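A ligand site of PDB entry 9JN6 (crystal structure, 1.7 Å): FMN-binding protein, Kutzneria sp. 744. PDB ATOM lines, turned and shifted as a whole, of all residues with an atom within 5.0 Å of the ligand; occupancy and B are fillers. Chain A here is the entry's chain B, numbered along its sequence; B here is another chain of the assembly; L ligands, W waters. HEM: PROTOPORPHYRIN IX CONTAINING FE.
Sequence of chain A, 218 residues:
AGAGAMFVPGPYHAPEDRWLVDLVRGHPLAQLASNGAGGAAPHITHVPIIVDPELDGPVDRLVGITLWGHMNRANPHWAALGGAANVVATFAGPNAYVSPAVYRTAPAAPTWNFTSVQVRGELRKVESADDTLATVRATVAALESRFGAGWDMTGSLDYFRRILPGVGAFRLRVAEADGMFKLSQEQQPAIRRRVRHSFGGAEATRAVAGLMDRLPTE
FE of the ligand is bound by NE2 of His 70 (2.0 Å).
N of Asn 72 sits at hydrogen-bond distance from O2A of the ligand (2.9 Å).
ND2 of Asn 75 sits at hydrogen-bond distance from O2A of the ligand, 3.1 Å away.
Water W5 lies within hydrogen-bond range of O1A of the ligand (2.7 Å) and O of His 46 (2.8 Å).
The side-chain amide nitrogen (ND2) of Asn 75 lies within hydrogen-bond range of the side-chain hydroxyl (OG1) of Thr 45.
OG1 of Thr 111 of chain B sits close to NZ of Lys 182 of chain B.
CG2 of Thr 45 touches O1A of the ligand, at 3.5 Å.
His 46 touches the ligand.
Pro 48 touches the ligand.
Met 71 touches the ligand (CB to O2A, 3.5 Å).
Val 136 touches the ligand (CB to C2C, 3.6 Å).
CG2 of Thr 139 touches CBB of the ligand, at 3.6 Å.
Val 140 touches the ligand (CG2 to CMC, 3.4 Å).
Leu 143 touches the ligand (CD1 to CMB, 3.97 Å).
Phe 160 touches the ligand.
O of Ile 163 touches CMD of the ligand (3.5 Å).
Leu 164 touches the ligand (CD1 to CBC, 3.9 Å).
Gly 166 touches the ligand (O to CAD, 3.7 Å).
Val 167 touches the ligand.
CB of Ala 109 of chain B touches CMC of the ligand, 3.99 Å away.
Pro 110 of chain B touches the ligand.
Thr 111 of chain B touches the ligand.
Trp 112 of chain B touches the ligand (CB to CMB, 3.7 Å).
Hydrophobic or aromatic side chains within 4 Å of the ligand: Pro 48, His 70, Met 71, Val 136, Val 140, Leu 143, Phe 160, Ile 163, Leu 164, Val 167, Ala 109 of chain B, Pro 110 of chain B and Trp 112 of chain B.
Within 4 Å of the ligand: Thr 45, His 46, Pro 48, His 70, Met 71, Asn 72, Asn 75, Val 136, Thr 139, Val 140, Leu 143, Phe 160, Ile 163, Leu 164, Gly 166, Val 167, Ala 109 of chain B, Pro 110 of chain B, Thr 111 of chain B and Trp 112 of chain B.
The nearest printed residue that does not touch the ligand is Tyr 97 of chain B (4.1 Å).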
ATOM      1  N   LEU A  29      -3.815  -6.316 -28.089  1.00  0.00           N
ATOM      2  CA  LEU A  29      -5.268  -6.501 -28.296  1.00  0.00           C
ATOM      3  C   LEU A  29      -5.455  -7.873 -28.964  1.00  0.00           C
ATOM      4  O   LEU A  29      -5.462  -7.976 -30.186  1.00  0.00           O
ATOM      5  CB  LEU A  29      -5.901  -5.335 -29.053  1.00  0.00           C
ATOM      6  CG  LEU A  29      -7.437  -5.341 -29.015  1.00  0.00           C
ATOM      7  CD1 LEU A  29      -7.924  -4.945 -27.641  1.00  0.00           C
ATOM      8  CD2 LEU A  29      -8.048  -4.451 -30.113  1.00  0.00           C
ATOM      9  N   THR A  45     -13.760 -12.462 -28.356  1.00  0.00           N
ATOM     10  CA  THR A  45     -13.705 -11.087 -27.861  1.00  0.00           C
ATOM     11  C   THR A  45     -12.307 -10.514 -28.011  1.00  0.00           C
ATOM     12  O   THR A  45     -11.346 -11.231 -27.634  1.00  0.00           O
ATOM     13  CB  THR A  45     -14.168 -11.009 -26.397  1.00  0.00           C
ATOM     14  OG1 THR A  45     -15.484 -11.583 -26.348  1.00  0.00           O
ATOM     15  CG2 THR A  45     -14.225  -9.555 -25.972  1.00  0.00           C
ATOM     16  N   HIS A  46     -12.223  -9.278 -28.534  1.00  0.00           N
ATOM     17  CA  HIS A  46     -10.956  -8.505 -28.513  1.00  0.00           C
ATOM     18  C   HIS A  46     -10.719  -7.946 -27.126  1.00  0.00           C
ATOM     19  O   HIS A  46     -11.548  -7.178 -26.640  1.00  0.00           O
ATOM     20  CB  HIS A  46     -10.926  -7.408 -29.528  1.00  0.00           C
ATOM     21  CG  HIS A  46     -10.896  -7.903 -30.915  1.00  0.00           C
ATOM     22  ND1 HIS A  46      -9.779  -7.915 -31.686  1.00  0.00           N
ATOM     23  CD2 HIS A  46     -11.883  -8.400 -31.666  1.00  0.00           C
ATOM     24  CE1 HIS A  46     -10.073  -8.413 -32.871  1.00  0.00           C
ATOM     25  NE2 HIS A  46     -11.364  -8.736 -32.874  1.00  0.00           N
ATOM     26  N   VAL A  47      -9.643  -8.364 -26.512  1.00  0.00           N
ATOM     27  CA  VAL A  47      -9.303  -7.989 -25.115  1.00  0.00           C
ATOM     28  C   VAL A  47      -7.833  -7.649 -25.000  1.00  0.00           C
ATOM     29  O   VAL A  47      -6.966  -8.288 -25.650  1.00  0.00           O
ATOM     30  CB  VAL A  47      -9.657  -9.143 -24.150  1.00  0.00           C
ATOM     31  CG1 VAL A  47     -11.146  -9.400 -24.121  1.00  0.00           C
ATOM     32  CG2 VAL A  47      -8.944 -10.451 -24.502  1.00  0.00           C
ATOM     33  N   PRO A  48      -7.553  -6.647 -24.166  1.00  0.00           N
ATOM     34  CA  PRO A  48      -6.162  -6.248 -23.915  1.00  0.00           C
ATOM     35  C   PRO A  48      -5.528  -7.238 -22.963  1.00  0.00           C
ATOM     36  O   PRO A  48      -6.036  -7.446 -21.826  1.00  0.00           O
ATOM     37  CB  PRO A  48      -6.282  -4.852 -23.283  1.00  0.00           C
ATOM     38  CG  PRO A  48      -7.655  -4.873 -22.628  1.00  0.00           C
ATOM     39  CD  PRO A  48      -8.523  -5.796 -23.451  1.00  0.00           C
ATOM     40  N   HIS A  70      -8.423  -8.080 -19.263  1.00  0.00           N
ATOM     41  CA  HIS A  70      -9.780  -7.718 -18.773  1.00  0.00           C
ATOM     42  C   HIS A  70     -10.747  -7.653 -19.955  1.00  0.00           C
ATOM     43  O   HIS A  70     -10.331  -7.518 -21.106  1.00  0.00           O
ATOM     44  CB  HIS A  70      -9.840  -6.424 -17.949  1.00  0.00           C
ATOM     45  CG  HIS A  70      -9.652  -5.127 -18.663  1.00  0.00           C
ATOM     46  ND1 HIS A  70      -8.396  -4.660 -19.009  1.00  0.00           N
ATOM     47  CD2 HIS A  70     -10.536  -4.171 -18.982  1.00  0.00           C
ATOM     48  CE1 HIS A  70      -8.510  -3.460 -19.571  1.00  0.00           C
ATOM     49  NE2 HIS A  70      -9.876  -3.091 -19.554  1.00  0.00           N
ATOM     50  N   MET A  71     -12.038  -7.636 -19.641  1.00  0.00           N
ATOM     51  CA  MET A  71     -13.095  -7.557 -20.661  1.00  0.00           C
ATOM     52  C   MET A  71     -14.283  -6.962 -19.919  1.00  0.00           C
ATOM     53  O   MET A  71     -14.141  -6.650 -18.740  1.00  0.00           O
ATOM     54  CB  MET A  71     -13.409  -8.937 -21.249  1.00  0.00           C
ATOM     55  CG  MET A  71     -14.070  -9.874 -20.302  1.00  0.00           C
ATOM     56  SD  MET A  71     -14.706 -11.333 -21.230  1.00  0.00           S
ATOM     57  CE  MET A  71     -13.189 -12.198 -21.193  1.00  0.00           C
ATOM     58  N   ASN A  72     -15.345  -6.743 -20.644  1.00  0.00           N
ATOM     59  CA  ASN A  72     -16.609  -6.173 -20.108  1.00  0.00           C
ATOM     60  C   ASN A  72     -17.420  -7.302 -19.442  1.00  0.00           C
ATOM     61  O   ASN A  72     -17.771  -8.265 -20.156  1.00  0.00           O
ATOM     62  CB  ASN A  72     -17.329  -5.535 -21.275  1.00  0.00           C
ATOM     63  CG  ASN A  72     -18.579  -4.797 -20.860  1.00  0.00           C
ATOM     64  OD1 ASN A  72     -18.932  -4.835 -19.718  1.00  0.00           O
ATOM     65  ND2 ASN A  72     -19.107  -4.020 -21.788  1.00  0.00           N
ATOM     66  N   ASN A  75     -20.558  -8.181 -21.410  1.00  0.00           N
ATOM     67  CA  ASN A  75     -20.349  -9.043 -22.585  1.00  0.00           C
ATOM     68  C   ASN A  75     -20.786 -10.456 -22.210  1.00  0.00           C
ATOM     69  O   ASN A  75     -20.194 -11.040 -21.315  1.00  0.00           O
ATOM     70  CB  ASN A  75     -18.855  -9.043 -22.966  1.00  0.00           C
ATOM     71  CG  ASN A  75     -18.548  -9.832 -24.219  1.00  0.00           C
ATOM     72  OD1 ASN A  75     -19.285 -10.733 -24.616  1.00  0.00           O
ATOM     73  ND2 ASN A  75     -17.405  -9.533 -24.799  1.00  0.00           N
ATOM     74  N   VAL A 136      -6.175  -3.316 -14.376  1.00  0.00           N
ATOM     75  CA  VAL A 136      -6.296  -2.167 -15.291  1.00  0.00           C
ATOM     76  C   VAL A 136      -5.146  -1.173 -15.082  1.00  0.00           C
ATOM     77  O   VAL A 136      -4.669  -0.652 -16.106  1.00  0.00           O
ATOM     78  CB  VAL A 136      -7.679  -1.455 -15.226  1.00  0.00           C
ATOM     79  CG1 VAL A 136      -8.797  -2.386 -15.640  1.00  0.00           C
ATOM     80  CG2 VAL A 136      -7.918  -0.832 -13.886  1.00  0.00           C
ATOM     81  N   THR A 139      -2.119  -2.582 -16.829  1.00  0.00           N
ATOM     82  CA  THR A 139      -2.365  -2.490 -18.291  1.00  0.00           C
ATOM     83  C   THR A 139      -2.062  -1.056 -18.719  1.00  0.00           C
ATOM     84  O   THR A 139      -1.453  -0.883 -19.777  1.00  0.00           O
ATOM     85  CB  THR A 139      -3.763  -2.975 -18.664  1.00  0.00           C
ATOM     86  OG1 THR A 139      -3.951  -4.319 -18.209  1.00  0.00           O
ATOM     87  CG2 THR A 139      -4.026  -2.873 -20.158  1.00  0.00           C
ATOM     88  N   VAL A 140      -2.501  -0.049 -17.980  1.00  0.00           N
ATOM     89  CA  VAL A 140      -2.159   1.357 -18.390  1.00  0.00           C
ATOM     90  C   VAL A 140      -0.638   1.419 -18.410  1.00  0.00           C
ATOM     91  O   VAL A 140      -0.078   2.009 -19.374  1.00  0.00           O
ATOM     92  CB  VAL A 140      -2.759   2.410 -17.466  1.00  0.00           C
ATOM     93  CG1 VAL A 140      -2.269   3.817 -17.843  1.00  0.00           C
ATOM     94  CG2 VAL A 140      -4.270   2.353 -17.494  1.00  0.00           C
ATOM     95  N   LEU A 143       0.843  -0.291 -21.447  1.00  0.00           N
ATOM     96  CA  LEU A 143       0.445   0.126 -22.831  1.00  0.00           C
ATOM     97  C   LEU A 143       0.789   1.607 -23.051  1.00  0.00           C
ATOM     98  O   LEU A 143       1.156   1.943 -24.168  1.00  0.00           O
ATOM     99  CB  LEU A 143      -1.028  -0.129 -23.149  1.00  0.00           C
ATOM    100  CG  LEU A 143      -1.577  -1.530 -23.081  1.00  0.00           C
ATOM    101  CD1 LEU A 143      -2.795  -1.711 -23.959  1.00  0.00           C
ATOM    102  CD2 LEU A 143      -0.581  -2.656 -23.180  1.00  0.00           C
ATOM    103  N   PHE A 160     -10.607   5.586 -11.889  1.00  0.00           N
ATOM    104  CA  PHE A 160     -10.599   4.150 -12.172  1.00  0.00           C
ATOM    105  C   PHE A 160     -11.463   3.403 -11.156  1.00  0.00           C
ATOM    106  O   PHE A 160     -12.170   2.467 -11.555  1.00  0.00           O
ATOM    107  CB  PHE A 160      -9.200   3.549 -12.119  1.00  0.00           C
ATOM    108  CG  PHE A 160      -8.217   4.057 -13.144  1.00  0.00           C
ATOM    109  CD1 PHE A 160      -8.594   4.878 -14.197  1.00  0.00           C
ATOM    110  CD2 PHE A 160      -6.918   3.600 -13.107  1.00  0.00           C
ATOM    111  CE1 PHE A 160      -7.666   5.299 -15.127  1.00  0.00           C
ATOM    112  CE2 PHE A 160      -5.982   4.000 -14.054  1.00  0.00           C
ATOM    113  CZ  PHE A 160      -6.367   4.836 -15.082  1.00  0.00           C
ATOM    114  N   ILE A 163     -15.206   3.848 -11.798  1.00  0.00           N
ATOM    115  CA  ILE A 163     -15.803   3.183 -12.991  1.00  0.00           C
ATOM    116  C   ILE A 163     -15.470   1.682 -12.976  1.00  0.00           C
ATOM    117  O   ILE A 163     -15.752   1.007 -13.981  1.00  0.00           O
ATOM    118  CB  ILE A 163     -15.352   3.865 -14.287  1.00  0.00           C
ATOM    119  CG1 ILE A 163     -13.843   3.810 -14.545  1.00  0.00           C
ATOM    120  CG2 ILE A 163     -15.846   5.263 -14.381  1.00  0.00           C
ATOM    121  CD1 ILE A 163     -13.514   3.845 -16.014  1.00  0.00           C
ATOM    122  N   LEU A 164     -15.059   1.109 -11.874  1.00  0.00           N
ATOM    123  CA  LEU A 164     -14.470  -0.271 -11.863  1.00  0.00           C
ATOM    124  C   LEU A 164     -15.458  -1.427 -12.016  1.00  0.00           C
ATOM    125  O   LEU A 164     -15.039  -2.515 -12.382  1.00  0.00           O
ATOM    126  CB  LEU A 164     -13.714  -0.494 -10.548  1.00  0.00           C
ATOM    127  CG  LEU A 164     -12.659  -1.606 -10.555  1.00  0.00           C
ATOM    128  CD1 LEU A 164     -11.510  -1.231 -11.474  1.00  0.00           C
ATOM    129  CD2 LEU A 164     -12.161  -1.877  -9.162  1.00  0.00           C
ATOM    130  N   GLY A 166     -17.698  -2.715 -13.953  1.00  0.00           N
ATOM    131  CA  GLY A 166     -17.954  -3.293 -15.267  1.00  0.00           C
ATOM    132  C   GLY A 166     -16.741  -4.078 -15.735  1.00  0.00           C
ATOM    133  O   GLY A 166     -16.897  -4.920 -16.613  1.00  0.00           O
ATOM    134  N   VAL A 167     -15.602  -3.893 -15.077  1.00  0.00           N
ATOM    135  CA  VAL A 167     -14.377  -4.685 -15.460  1.00  0.00           C
ATOM    136  C   VAL A 167     -14.489  -6.148 -15.034  1.00  0.00           C
ATOM    137  O   VAL A 167     -14.626  -6.437 -13.828  1.00  0.00           O
ATOM    138  CB  VAL A 167     -13.131  -4.049 -14.841  1.00  0.00           C
ATOM    139  CG1 VAL A 167     -11.883  -4.840 -15.262  1.00  0.00           C
ATOM    140  CG2 VAL A 167     -13.046  -2.600 -15.228  1.00  0.00           C
ATOM    141  N   PHE B   7     -20.661  -9.548 -29.014  1.00  0.00           N
ATOM    142  CA  PHE B   7     -21.144  -8.412 -28.197  1.00  0.00           C
ATOM    143  C   PHE B   7     -20.617  -7.099 -28.791  1.00  0.00           C
ATOM    144  O   PHE B   7     -19.379  -6.859 -28.769  1.00  0.00           O
ATOM    145  CB  PHE B   7     -20.672  -8.549 -26.748  1.00  0.00           C
ATOM    146  CG  PHE B   7     -21.156  -7.414 -25.893  1.00  0.00           C
ATOM    147  CD1 PHE B   7     -22.506  -7.234 -25.668  1.00  0.00           C
ATOM    148  CD2 PHE B   7     -20.259  -6.508 -25.354  1.00  0.00           C
ATOM    149  CE1 PHE B   7     -22.958  -6.190 -24.873  1.00  0.00           C
ATOM    150  CE2 PHE B   7     -20.710  -5.457 -24.567  1.00  0.00           C
ATOM    151  CZ  PHE B   7     -22.067  -5.303 -24.324  1.00  0.00           C
ATOM    152  N   TYR B  97      -4.113   2.321 -30.433  1.00  0.00           N
ATOM    153  CA  TYR B  97      -4.130   2.724 -29.018  1.00  0.00           C
ATOM    154  C   TYR B  97      -4.520   4.188 -28.873  1.00  0.00           C
ATOM    155  O   TYR B  97      -4.035   5.031 -29.634  1.00  0.00           O
ATOM    156  CB  TYR B  97      -2.785   2.428 -28.369  1.00  0.00           C
ATOM    157  CG  TYR B  97      -2.775   2.840 -26.918  1.00  0.00           C
ATOM    158  CD1 TYR B  97      -3.344   2.058 -25.931  1.00  0.00           C
ATOM    159  CD2 TYR B  97      -2.164   4.017 -26.547  1.00  0.00           C
ATOM    160  CE1 TYR B  97      -3.294   2.443 -24.604  1.00  0.00           C
ATOM    161  CE2 TYR B  97      -2.095   4.418 -25.219  1.00  0.00           C
ATOM    162  CZ  TYR B  97      -2.652   3.621 -24.243  1.00  0.00           C
ATOM    163  OH  TYR B  97      -2.537   3.962 -22.936  1.00  0.00           O
ATOM    164  N   ALA B 109      -9.570   7.295 -18.937  1.00  0.00           N
ATOM    165  CA  ALA B 109      -8.863   6.016 -19.020  1.00  0.00           C
ATOM    166  C   ALA B 109      -8.533   5.791 -20.482  1.00  0.00           C
ATOM    167  O   ALA B 109      -9.280   6.199 -21.373  1.00  0.00           O
ATOM    168  CB  ALA B 109      -9.699   4.915 -18.435  1.00  0.00           C
ATOM    169  N   PRO B 110      -7.394   5.173 -20.805  1.00  0.00           N
ATOM    170  CA  PRO B 110      -7.115   4.827 -22.187  1.00  0.00           C
ATOM    171  C   PRO B 110      -8.064   3.762 -22.742  1.00  0.00           C
ATOM    172  O   PRO B 110      -8.744   3.038 -22.047  1.00  0.00           O
ATOM    173  CB  PRO B 110      -5.711   4.215 -22.143  1.00  0.00           C
ATOM    174  CG  PRO B 110      -5.195   4.534 -20.757  1.00  0.00           C
ATOM    175  CD  PRO B 110      -6.408   4.609 -19.874  1.00  0.00           C
ATOM    176  N   THR B 111      -8.005   3.589 -24.058  1.00  0.00           N
ATOM    177  CA  THR B 111      -8.648   2.435 -24.709  1.00  0.00           C
ATOM    178  C   THR B 111      -7.919   2.072 -26.007  1.00  0.00           C
ATOM    179  O   THR B 111      -6.762   2.531 -26.262  1.00  0.00           O
ATOM    180  CB  THR B 111     -10.128   2.741 -24.892  1.00  0.00           C
ATOM    181  OG1 THR B 111     -10.820   1.535 -25.266  1.00  0.00           O
ATOM    182  CG2 THR B 111     -10.329   3.762 -25.992  1.00  0.00           C
ATOM    183  N   TRP B 112      -8.514   1.144 -26.718  1.00  0.00           N
ATOM    184  CA  TRP B 112      -7.947   0.751 -28.021  1.00  0.00           C
ATOM    185  C   TRP B 112      -9.079   0.843 -29.047  1.00  0.00           C
ATOM    186  O   TRP B 112     -10.091   0.211 -28.850  1.00  0.00           O
ATOM    187  CB  TRP B 112      -7.309  -0.644 -27.982  1.00  0.00           C
ATOM    188  CG  TRP B 112      -6.249  -0.864 -29.004  1.00  0.00           C
ATOM    189  CD1 TRP B 112      -6.397  -0.962 -30.359  1.00  0.00           C
ATOM    190  CD2 TRP B 112      -4.872  -1.052 -28.769  1.00  0.00           C
ATOM    191  NE1 TRP B 112      -5.194  -1.198 -30.974  1.00  0.00           N
ATOM    192  CE2 TRP B 112      -4.230  -1.266 -30.013  1.00  0.00           C
ATOM    193  CE3 TRP B 112      -4.091  -1.062 -27.602  1.00  0.00           C
ATOM    194  CZ2 TRP B 112      -2.851  -1.492 -30.120  1.00  0.00           C
ATOM    195  CZ3 TRP B 112      -2.748  -1.283 -27.720  1.00  0.00           C
ATOM    196  CH2 TRP B 112      -2.121  -1.430 -28.961  1.00  0.00           C
ATOM    197  N   PHE B 114     -10.607  -0.084 -32.556  1.00  0.00           N
ATOM    198  CA  PHE B 114     -10.381  -1.190 -33.477  1.00  0.00           C
ATOM    199  C   PHE B 114     -11.654  -1.483 -34.230  1.00  0.00           C
ATOM    200  O   PHE B 114     -12.801  -1.029 -33.848  1.00  0.00           O
ATOM    201  CB  PHE B 114      -9.871  -2.407 -32.716  1.00  0.00           C
ATOM    202  CG  PHE B 114     -10.928  -3.111 -31.907  1.00  0.00           C
ATOM    203  CD1 PHE B 114     -11.184  -2.762 -30.599  1.00  0.00           C
ATOM    204  CD2 PHE B 114     -11.584  -4.225 -32.437  1.00  0.00           C
ATOM    205  CE1 PHE B 114     -12.107  -3.488 -29.840  1.00  0.00           C
ATOM    206  CE2 PHE B 114     -12.548  -4.894 -31.711  1.00  0.00           C
ATOM    207  CZ  PHE B 114     -12.808  -4.528 -30.402  1.00  0.00           C
ATOM    208  N   MET B 180     -17.914  -4.658 -35.032  1.00  0.00           N
ATOM    209  CA  MET B 180     -17.399  -3.768 -33.982  1.00  0.00           C
ATOM    210  C   MET B 180     -16.677  -2.627 -34.694  1.00  0.00           C
ATOM    211  O   MET B 180     -15.576  -2.862 -35.313  1.00  0.00           O
ATOM    212  CB  MET B 180     -16.422  -4.506 -33.052  1.00  0.00           C
ATOM    213  CG  MET B 180     -15.770  -3.651 -32.023  1.00  0.00           C
ATOM    214  SD  MET B 180     -16.838  -3.236 -30.609  1.00  0.00           S
ATOM    215  CE  MET B 180     -16.853  -4.841 -29.816  1.00  0.00           C
ATOM    216  N   LYS B 182     -15.166   0.334 -33.155  1.00  0.00           N
ATOM    217  CA  LYS B 182     -14.893   0.995 -31.864  1.00  0.00           C
ATOM    218  C   LYS B 182     -14.024   2.193 -32.186  1.00  0.00           C
ATOM    219  O   LYS B 182     -12.758   2.030 -32.415  1.00  0.00           O
ATOM    220  CB  LYS B 182     -14.316   0.036 -30.849  1.00  0.00           C
ATOM    221  CG  LYS B 182     -13.870   0.735 -29.571  1.00  0.00           C
ATOM    222  CD  LYS B 182     -13.556  -0.176 -28.413  1.00  0.00           C
ATOM    223  CE  LYS B 182     -12.827   0.618 -27.340  1.00  0.00           C
ATOM    224  NZ  LYS B 182     -13.731   1.542 -26.626  1.00  0.00           N
HETATM  225  CHA HEM L   1     -13.681  -3.028 -21.235  1.00  0.00           C
HETATM  226  CHB HEM L   1      -9.496  -2.086 -23.498  1.00  0.00           C
HETATM  227  CHC HEM L   1      -7.810   0.327 -19.606  1.00  0.00           C
HETATM  228  CHD HEM L   1     -12.237  -0.013 -17.586  1.00  0.00           C
HETATM  229  C1A HEM L   1     -12.640  -3.069 -22.138  1.00  0.00           C
HETATM  230  C2A HEM L   1     -12.766  -3.559 -23.489  1.00  0.00           C
HETATM  231  C3A HEM L   1     -11.575  -3.305 -24.143  1.00  0.00           C
HETATM  232  C4A HEM L   1     -10.757  -2.552 -23.202  1.00  0.00           C
HETATM  233  CMA HEM L   1     -11.289  -3.712 -25.600  1.00  0.00           C
HETATM  234  CAA HEM L   1     -13.952  -4.338 -24.041  1.00  0.00           C
HETATM  235  CBA HEM L   1     -13.845  -5.838 -23.841  1.00  0.00           C
HETATM  236  CGA HEM L   1     -15.126  -6.527 -24.246  1.00  0.00           C
HETATM  237  O1A HEM L   1     -15.667  -6.364 -25.406  1.00  0.00           O
HETATM  238  O2A HEM L   1     -15.606  -7.341 -23.436  1.00  0.00           O
HETATM  239  C1B HEM L   1      -8.699  -1.326 -22.670  1.00  0.00           C
HETATM  240  C2B HEM L   1      -7.387  -0.900 -22.996  1.00  0.00           C
HETATM  241  C3B HEM L   1      -6.886  -0.210 -21.929  1.00  0.00           C
HETATM  242  C4B HEM L   1      -7.917  -0.220 -20.887  1.00  0.00           C
HETATM  243  CMB HEM L   1      -6.700  -1.130 -24.329  1.00  0.00           C
HETATM  244  CAB HEM L   1      -5.517   0.338 -21.920  1.00  0.00           C
HETATM  245  CBB HEM L   1      -4.796   0.558 -20.903  1.00  0.00           C
HETATM  246  C1C HEM L   1      -8.869   0.454 -18.737  1.00  0.00           C
HETATM  247  C2C HEM L   1      -8.827   1.120 -17.505  1.00  0.00           C
HETATM  248  C3C HEM L   1     -10.098   1.064 -16.912  1.00  0.00           C
HETATM  249  C4C HEM L   1     -10.888   0.244 -17.815  1.00  0.00           C
HETATM  250  CMC HEM L   1      -7.630   1.842 -16.947  1.00  0.00           C
HETATM  251  CAC HEM L   1     -10.432   1.559 -15.553  1.00  0.00           C
HETATM  252  CBC HEM L   1     -11.288   0.957 -14.716  1.00  0.00           C
HETATM  253  C1D HEM L   1     -12.960  -0.819 -18.474  1.00  0.00           C
HETATM  254  C2D HEM L   1     -14.357  -1.075 -18.259  1.00  0.00           C
HETATM  255  C3D HEM L   1     -14.745  -1.912 -19.195  1.00  0.00           C
HETATM  256  C4D HEM L   1     -13.570  -2.232 -20.074  1.00  0.00           C
HETATM  257  CMD HEM L   1     -15.235  -0.567 -17.095  1.00  0.00           C
HETATM  258  CAD HEM L   1     -16.172  -2.490 -19.348  1.00  0.00           C
HETATM  259  CBD HEM L   1     -16.894  -1.908 -20.587  1.00  0.00           C
HETATM  260  CGD HEM L   1     -16.801  -0.415 -20.718  1.00  0.00           C
HETATM  261  O1D HEM L   1     -17.253   0.261 -19.772  1.00  0.00           O
HETATM  262  O2D HEM L   1     -16.247   0.128 -21.709  1.00  0.00           O
HETATM  263  NA  HEM L   1     -11.426  -2.370 -22.038  1.00  0.00           N
HETATM  264  NB  HEM L   1      -8.913  -1.033 -21.367  1.00  0.00           N
HETATM  265  NC  HEM L   1     -10.102  -0.110 -18.909  1.00  0.00           N
HETATM  266  ND  HEM L   1     -12.514  -1.483 -19.604  1.00  0.00           N
HETATM  267 FE   HEM L   1     -10.718  -1.441 -20.390  1.00  0.00          FE
HETATM  268  O   HOH W   1     -18.659  -0.669 -17.691  1.00  0.00           O
HETATM  269  O   HOH W   2     -11.882   0.791 -22.744  1.00  0.00           O
HETATM  270  O   HOH W   3     -14.544  -0.555 -23.842  1.00  0.00           O
HETATM  271  O   HOH W   4     -16.560   2.505 -23.399  1.00  0.00           O
HETATM  272  O   HOH W   5     -13.868  -5.902 -27.387  1.00  0.00           O
